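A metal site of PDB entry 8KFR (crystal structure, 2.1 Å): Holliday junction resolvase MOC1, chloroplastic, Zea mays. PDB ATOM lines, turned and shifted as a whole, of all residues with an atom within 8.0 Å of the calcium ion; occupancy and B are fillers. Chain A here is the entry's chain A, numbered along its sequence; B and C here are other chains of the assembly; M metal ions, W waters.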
ATOM      1  N   VAL A   6       8.539  12.294  -5.641  1.00  0.00           N
ATOM      2  CA  VAL A   6       7.693  11.391  -6.407  1.00  0.00           C
ATOM      3  C   VAL A   6       7.305  12.041  -7.737  1.00  0.00           C
ATOM      4  O   VAL A   6       6.666  13.099  -7.769  1.00  0.00           O
ATOM      5  CB  VAL A   6       6.436  10.977  -5.642  1.00  0.00           C
ATOM      6  CG1 VAL A   6       5.480  10.254  -6.583  1.00  0.00           C
ATOM      7  CG2 VAL A   6       6.815  10.065  -4.454  1.00  0.00           C
ATOM      8  N   ASP A   7       7.708  11.398  -8.835  1.00  0.00           N
ATOM      9  CA  ASP A   7       7.144  11.647 -10.148  1.00  0.00           C
ATOM     10  C   ASP A   7       6.043  10.626 -10.352  1.00  0.00           C
ATOM     11  O   ASP A   7       6.354   9.438 -10.564  1.00  0.00           O
ATOM     12  CB  ASP A   7       8.215  11.504 -11.230  1.00  0.00           C
ATOM     13  CG  ASP A   7       7.668  11.732 -12.621  1.00  0.00           C
ATOM     14  OD1 ASP A   7       6.585  12.338 -12.761  1.00  0.00           O
ATOM     15  OD2 ASP A   7       8.312  11.287 -13.587  1.00  0.00           O
ATOM     16  N   PRO A   8       4.760  11.008 -10.276  1.00  0.00           N
ATOM     17  CA  PRO A   8       3.696  10.003 -10.101  1.00  0.00           C
ATOM     18  C   PRO A   8       3.224   9.307 -11.373  1.00  0.00           C
ATOM     19  O   PRO A   8       2.413   8.386 -11.246  1.00  0.00           O
ATOM     20  CB  PRO A   8       2.557  10.815  -9.472  1.00  0.00           C
ATOM     21  CG  PRO A   8       2.792  12.221  -9.935  1.00  0.00           C
ATOM     22  CD  PRO A   8       4.275  12.389 -10.076  1.00  0.00           C
ATOM     23  N   ASP A   9       3.688   9.705 -12.563  1.00  0.00           N
ATOM     24  CA  ASP A   9       3.112   9.141 -13.777  1.00  0.00           C
ATOM     25  C   ASP A   9       3.618   7.718 -14.015  1.00  0.00           C
ATOM     26  O   ASP A   9       4.412   7.169 -13.257  1.00  0.00           O
ATOM     27  CB  ASP A   9       3.359  10.035 -14.995  1.00  0.00           C
ATOM     28  CG  ASP A   9       4.823  10.393 -15.199  1.00  0.00           C
ATOM     29  OD1 ASP A   9       5.628   9.488 -15.549  1.00  0.00           O
ATOM     30  OD2 ASP A   9       5.160  11.591 -15.084  1.00  0.00           O
ATOM     31  N   ILE A  10       3.105   7.106 -15.100  1.00  0.00           N
ATOM     32  CA  ILE A  10       3.344   5.690 -15.372  1.00  0.00           C
ATOM     33  C   ILE A  10       4.824   5.440 -15.675  1.00  0.00           C
ATOM     34  O   ILE A  10       5.344   4.352 -15.376  1.00  0.00           O
ATOM     35  CB  ILE A  10       2.429   5.201 -16.519  1.00  0.00           C
ATOM     36  CG1 ILE A  10       2.193   3.702 -16.409  1.00  0.00           C
ATOM     37  CG2 ILE A  10       3.000   5.496 -17.907  1.00  0.00           C
ATOM     38  CD1 ILE A  10       1.355   3.365 -15.207  1.00  0.00           C
ATOM     39  N   GLY A  11       5.537   6.420 -16.217  1.00  0.00           N
ATOM     40  CA  GLY A  11       6.954   6.260 -16.437  1.00  0.00           C
ATOM     41  C   GLY A  11       7.742   6.958 -15.347  1.00  0.00           C
ATOM     42  O   GLY A  11       8.939   7.217 -15.504  1.00  0.00           O
ATOM     43  N   GLY A  12       7.077   7.268 -14.243  1.00  0.00           N
ATOM     44  CA  GLY A  12       7.692   8.003 -13.154  1.00  0.00           C
ATOM     45  C   GLY A  12       8.526   7.138 -12.240  1.00  0.00           C
ATOM     46  O   GLY A  12       8.929   6.016 -12.582  1.00  0.00           O
ATOM     47  N   ALA A  13       8.775   7.665 -11.028  1.00  0.00           N
ATOM     48  CA  ALA A  13       9.743   7.086 -10.116  1.00  0.00           C
ATOM     49  C   ALA A  13       9.554   7.715  -8.739  1.00  0.00           C
ATOM     50  O   ALA A  13       8.993   8.817  -8.609  1.00  0.00           O
ATOM     51  CB  ALA A  13      11.182   7.308 -10.595  1.00  0.00           C
ATOM     52  N   ASN A  28       8.448   3.482 -11.011  1.00  0.00           N
ATOM     53  CA  ASN A  28       7.105   3.234 -10.500  1.00  0.00           C
ATOM     54  C   ASN A  28       6.660   1.848 -10.951  1.00  0.00           C
ATOM     55  O   ASN A  28       6.694   1.563 -12.147  1.00  0.00           O
ATOM     56  CB  ASN A  28       6.118   4.288 -10.990  1.00  0.00           C
ATOM     57  CG  ASN A  28       6.282   5.632 -10.283  1.00  0.00           C
ATOM     58  OD1 ASN A  28       7.006   5.754  -9.291  1.00  0.00           O
ATOM     59  ND2 ASN A  28       5.606   6.644 -10.793  1.00  0.00           N
ATOM     60  N   GLU A  66       5.015  15.805  -7.669  1.00  0.00           N
ATOM     61  CA  GLU A  66       4.691  16.748  -8.729  1.00  0.00           C
ATOM     62  C   GLU A  66       3.178  16.861  -8.855  1.00  0.00           C
ATOM     63  O   GLU A  66       2.479  15.858  -9.026  1.00  0.00           O
ATOM     64  CB  GLU A  66       5.315  16.308 -10.040  1.00  0.00           C
ATOM     65  CG  GLU A  66       5.045  17.316 -11.144  1.00  0.00           C
ATOM     66  CD  GLU A  66       5.920  17.082 -12.341  1.00  0.00           C
ATOM     67  OE1 GLU A  66       7.100  17.497 -12.289  1.00  0.00           O
ATOM     68  OE2 GLU A  66       5.415  16.463 -13.324  1.00  0.00           O
ATOM     69  N   TRP A 108      10.197  23.427  -9.455  1.00  0.00           N
ATOM     70  CA  TRP A 108      11.523  22.806  -9.375  1.00  0.00           C
ATOM     71  C   TRP A 108      12.309  23.036 -10.644  1.00  0.00           C
ATOM     72  O   TRP A 108      13.542  23.113 -10.595  1.00  0.00           O
ATOM     73  CB  TRP A 108      11.438  21.305  -9.054  1.00  0.00           C
ATOM     74  CG  TRP A 108      10.743  20.413 -10.041  1.00  0.00           C
ATOM     75  CD1 TRP A 108       9.438  19.995 -10.009  1.00  0.00           C
ATOM     76  CD2 TRP A 108      11.330  19.768 -11.186  1.00  0.00           C
ATOM     77  NE1 TRP A 108       9.171  19.163 -11.072  1.00  0.00           N
ATOM     78  CE2 TRP A 108      10.320  19.002 -11.811  1.00  0.00           C
ATOM     79  CE3 TRP A 108      12.616  19.773 -11.755  1.00  0.00           C
ATOM     80  CZ2 TRP A 108      10.553  18.262 -12.961  1.00  0.00           C
ATOM     81  CZ3 TRP A 108      12.843  19.040 -12.906  1.00  0.00           C
ATOM     82  CH2 TRP A 108      11.821  18.295 -13.503  1.00  0.00           C
ATOM     83  N   LYS A 121      13.940  16.752 -21.215  1.00  0.00           N
ATOM     84  CA  LYS A 121      14.137  15.480 -20.535  1.00  0.00           C
ATOM     85  C   LYS A 121      15.621  15.146 -20.403  1.00  0.00           C
ATOM     86  O   LYS A 121      16.053  14.666 -19.339  1.00  0.00           O
ATOM     87  CB  LYS A 121      13.380  14.381 -21.278  1.00  0.00           C
ATOM     88  CG  LYS A 121      11.857  14.580 -21.234  1.00  0.00           C
ATOM     89  CD  LYS A 121      11.143  13.348 -21.790  1.00  0.00           C
ATOM     90  CE  LYS A 121       9.630  13.505 -21.815  1.00  0.00           C
ATOM     91  NZ  LYS A 121       9.016  12.262 -22.369  1.00  0.00           N
ATOM     92  N   HIS A 145      14.203   9.570 -17.614  1.00  0.00           N
ATOM     93  CA  HIS A 145      13.900  10.935 -17.220  1.00  0.00           C
ATOM     94  C   HIS A 145      12.913  10.989 -16.057  1.00  0.00           C
ATOM     95  O   HIS A 145      12.865  12.009 -15.356  1.00  0.00           O
ATOM     96  CB  HIS A 145      13.348  11.708 -18.410  1.00  0.00           C
ATOM     97  CG  HIS A 145      11.992  11.259 -18.858  1.00  0.00           C
ATOM     98  ND1 HIS A 145      10.831  11.823 -18.393  1.00  0.00           N
ATOM     99  CD2 HIS A 145      11.614  10.305 -19.754  1.00  0.00           C
ATOM    100  CE1 HIS A 145       9.788  11.233 -18.962  1.00  0.00           C
ATOM    101  NE2 HIS A 145      10.242  10.316 -19.791  1.00  0.00           N
ATOM    102  N   GLY A 146      12.130   9.935 -15.836  1.00  0.00           N
ATOM    103  CA  GLY A 146      11.286   9.895 -14.654  1.00  0.00           C
ATOM    104  C   GLY A 146      12.105   9.702 -13.389  1.00  0.00           C
ATOM    105  O   GLY A 146      11.848  10.356 -12.373  1.00  0.00           O
ATOM    106  N   ARG A 147      13.113   8.831 -13.440  1.00  0.00           N
ATOM    107  CA  ARG A 147      14.080   8.727 -12.347  1.00  0.00           C
ATOM    108  C   ARG A 147      14.723  10.069 -12.041  1.00  0.00           C
ATOM    109  O   ARG A 147      14.919  10.403 -10.876  1.00  0.00           O
ATOM    110  CB  ARG A 147      15.163   7.723 -12.671  1.00  0.00           C
ATOM    111  CG  ARG A 147      14.676   6.302 -12.846  1.00  0.00           C
ATOM    112  CD  ARG A 147      15.827   5.427 -13.282  1.00  0.00           C
ATOM    113  NE  ARG A 147      15.394   4.063 -13.550  1.00  0.00           N
ATOM    114  CZ  ARG A 147      16.210   3.080 -13.909  1.00  0.00           C
ATOM    115  NH1 ARG A 147      17.510   3.278 -14.023  1.00  0.00           N
ATOM    116  NH2 ARG A 147      15.697   1.869 -14.147  1.00  0.00           N
ATOM    117  N   GLU A 149      13.485  13.208 -12.694  1.00  0.00           N
ATOM    118  CA  GLU A 149      12.500  14.124 -12.166  1.00  0.00           C
ATOM    119  C   GLU A 149      12.211  13.830 -10.701  1.00  0.00           C
ATOM    120  O   GLU A 149      12.100  14.756  -9.878  1.00  0.00           O
ATOM    121  CB  GLU A 149      11.219  14.064 -13.008  1.00  0.00           C
ATOM    122  CG  GLU A 149      11.373  14.722 -14.389  1.00  0.00           C
ATOM    123  CD  GLU A 149      10.567  14.060 -15.512  1.00  0.00           C
ATOM    124  OE1 GLU A 149       9.770  13.126 -15.273  1.00  0.00           O
ATOM    125  OE2 GLU A 149      10.749  14.471 -16.678  1.00  0.00           O
ATOM    126  N   ALA A 150      12.101  12.555 -10.343  1.00  0.00           N
ATOM    127  CA  ALA A 150      11.886  12.200  -8.939  1.00  0.00           C
ATOM    128  C   ALA A 150      13.069  12.638  -8.090  1.00  0.00           C
ATOM    129  O   ALA A 150      12.877  13.210  -7.005  1.00  0.00           O
ATOM    130  CB  ALA A 150      11.652  10.708  -8.789  1.00  0.00           C
ATOM    131  N   LEU A 153      12.931  16.462  -7.794  1.00  0.00           N
ATOM    132  CA  LEU A 153      11.916  16.869  -6.826  1.00  0.00           C
ATOM    133  C   LEU A 153      12.422  16.718  -5.409  1.00  0.00           C
ATOM    134  O   LEU A 153      12.246  17.621  -4.574  1.00  0.00           O
ATOM    135  CB  LEU A 153      10.636  16.041  -7.002  1.00  0.00           C
ATOM    136  CG  LEU A 153       9.711  16.478  -8.110  1.00  0.00           C
ATOM    137  CD1 LEU A 153       8.935  15.288  -8.634  1.00  0.00           C
ATOM    138  CD2 LEU A 153       8.772  17.544  -7.585  1.00  0.00           C
ATOM    139  OP3  DC B   1       6.340  14.893 -19.296  1.00  0.00           O
ATOM    140  P    DC B   1       6.106  13.644 -18.540  1.00  0.00           P
ATOM    141  OP1  DC B   1       6.377  13.903 -17.113  1.00  0.00           O
ATOM    142  OP2  DC B   1       6.848  12.566 -19.241  1.00  0.00           O
ATOM    143  O5'  DC B   1       4.565  13.275 -18.679  1.00  0.00           O
ATOM    144  C5'  DC B   1       3.763  13.143 -17.523  1.00  0.00           C
ATOM    145  C4'  DC B   1       2.313  12.982 -17.912  1.00  0.00           C
ATOM    146  O4'  DC B   1       1.947  14.065 -18.796  1.00  0.00           O
ATOM    147  C3'  DC B   1       2.015  11.705 -18.698  1.00  0.00           C
ATOM    148  O3'  DC B   1       1.594  10.685 -17.815  1.00  0.00           O
ATOM    149  C2'  DC B   1       0.864  12.123 -19.593  1.00  0.00           C
ATOM    150  C1'  DC B   1       1.006  13.619 -19.745  1.00  0.00           C
ATOM    151  N1   DC B   1       1.414  14.036 -21.114  1.00  0.00           N
ATOM    152  C2   DC B   1       0.450  14.006 -22.146  1.00  0.00           C
ATOM    153  O2   DC B   1      -0.694  13.629 -21.881  1.00  0.00           O
ATOM    154  N3   DC B   1       0.798  14.422 -23.382  1.00  0.00           N
ATOM    155  C4   DC B   1       2.068  14.803 -23.630  1.00  0.00           C
ATOM    156  N4   DC B   1       2.361  15.175 -24.873  1.00  0.00           N
ATOM    157  C5   DC B   1       3.061  14.820 -22.604  1.00  0.00           C
ATOM    158  C6   DC B   1       2.698  14.432 -21.371  1.00  0.00           C
ATOM    159  P    DA B   2       1.508   9.146 -18.301  1.00  0.00           P
ATOM    160  OP1  DA B   2       1.211   8.328 -17.099  1.00  0.00           O
ATOM    161  OP2  DA B   2       2.714   8.851 -19.072  1.00  0.00           O
ATOM    162  O5'  DA B   2       0.246   9.072 -19.281  1.00  0.00           O
ATOM    163  C5'  DA B   2      -1.082   9.320 -18.777  1.00  0.00           C
ATOM    164  C4'  DA B   2      -2.120   9.104 -19.859  1.00  0.00           C
ATOM    165  O4'  DA B   2      -1.906   9.991 -20.981  1.00  0.00           O
ATOM    166  C3'  DA B   2      -2.171   7.693 -20.421  1.00  0.00           C
ATOM    167  O3'  DA B   2      -3.529   7.322 -20.597  1.00  0.00           O
ATOM    168  C2'  DA B   2      -1.431   7.808 -21.757  1.00  0.00           C
ATOM    169  C1'  DA B   2      -1.710   9.249 -22.176  1.00  0.00           C
ATOM    170  N9   DA B   2      -0.595   9.872 -22.878  1.00  0.00           N
ATOM    171  C8   DA B   2       0.637  10.127 -22.366  1.00  0.00           C
ATOM    172  N7   DA B   2       1.433  10.748 -23.190  1.00  0.00           N
ATOM    173  C5   DA B   2       0.660  10.935 -24.319  1.00  0.00           C
ATOM    174  C6   DA B   2       0.953  11.527 -25.551  1.00  0.00           C
ATOM    175  N6   DA B   2       2.137  12.061 -25.831  1.00  0.00           N
ATOM    176  N1   DA B   2      -0.039  11.553 -26.486  1.00  0.00           N
ATOM    177  C2   DA B   2      -1.218  10.998 -26.185  1.00  0.00           C
ATOM    178  N3   DA B   2      -1.599  10.418 -25.045  1.00  0.00           N
ATOM    179  C4   DA B   2      -0.594  10.413 -24.158  1.00  0.00           C
ATOM    180  P    DC C  25       7.814  20.359 -19.365  1.00  0.00           P
ATOM    181  OP1  DC C  25       9.063  19.737 -18.901  1.00  0.00           O
ATOM    182  OP2  DC C  25       7.833  21.268 -20.532  1.00  0.00           O
ATOM    183  O5'  DC C  25       6.794  19.184 -19.709  1.00  0.00           O
ATOM    184  C5'  DC C  25       6.650  18.121 -18.811  1.00  0.00           C
ATOM    185  C4'  DC C  25       5.489  18.382 -17.892  1.00  0.00           C
ATOM    186  O4'  DC C  25       4.414  18.937 -18.686  1.00  0.00           O
ATOM    187  C3'  DC C  25       4.926  17.159 -17.189  1.00  0.00           C
ATOM    188  O3'  DC C  25       4.485  17.526 -15.895  1.00  0.00           O
ATOM    189  C2'  DC C  25       3.773  16.742 -18.105  1.00  0.00           C
ATOM    190  C1'  DC C  25       3.287  18.100 -18.611  1.00  0.00           C
ATOM    191  N1   DC C  25       2.636  18.063 -19.966  1.00  0.00           N
ATOM    192  C2   DC C  25       1.290  17.700 -20.070  1.00  0.00           C
ATOM    193  O2   DC C  25       0.667  17.403 -19.051  1.00  0.00           O
ATOM    194  N3   DC C  25       0.704  17.694 -21.275  1.00  0.00           N
ATOM    195  C4   DC C  25       1.386  18.014 -22.366  1.00  0.00           C
ATOM    196  N4   DC C  25       0.732  17.971 -23.530  1.00  0.00           N
ATOM    197  C5   DC C  25       2.764  18.392 -22.298  1.00  0.00           C
ATOM    198  C6   DC C  25       3.334  18.412 -21.085  1.00  0.00           C
HETATM  199 CA    CA M   1       7.258  12.427 -15.276  1.00  0.00          CA
HETATM  200  O   HOH W   1       5.318  14.166 -14.276  1.00  0.00           O
HETATM  201  O   HOH W   2       7.794  10.663 -16.336  1.00  0.00           O
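Of the 21 residues printed, 4 come within 4 Å of the calcium ion.
OP2 of DC 1 of chain B lies within salt-bridge range of the side-chain amino group of Lys 121 (3.8 Å). The backbone NH (N) of Gly 11 sits at hydrogen-bond distance from the side-chain carboxylate (OD1) of Asp 9, at 3.1 Å. OE2 of Glu 149 lies within hydrogen-bond range of ND1 of His 145 (3.2 Å). The backbone NH (N) of Asp 7 is in hydrogen-bond range of the backbone carbonyl oxygen (O) of Ala 13, 2.9 Å away. The side-chain carboxylate (OD1) of Asp 9 is in hydrogen-bond range of the backbone NH (N) of Gly 12. ND2 of Asn 28 sits at hydrogen-bond distance from O of Asp 7, at 2.9 Å. The backbone carbonyl oxygen (O) of Asp 9 sits at hydrogen-bond distance from the side-chain amide nitrogen (ND2) of Asn 28 (2.8 Å).
The calcium ion is bound by water W2, the side-chain carboxylate (OD2) of Asp 9, the side-chain carboxylate (OD2) of Asp 7, OP1 of DC 1 of chain B, the side-chain carboxylate (OD1) of Asp 7, the side-chain carboxylate (OE1) of Glu 149 and water W1. The calcium ion has seven donor atoms within binding distance.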
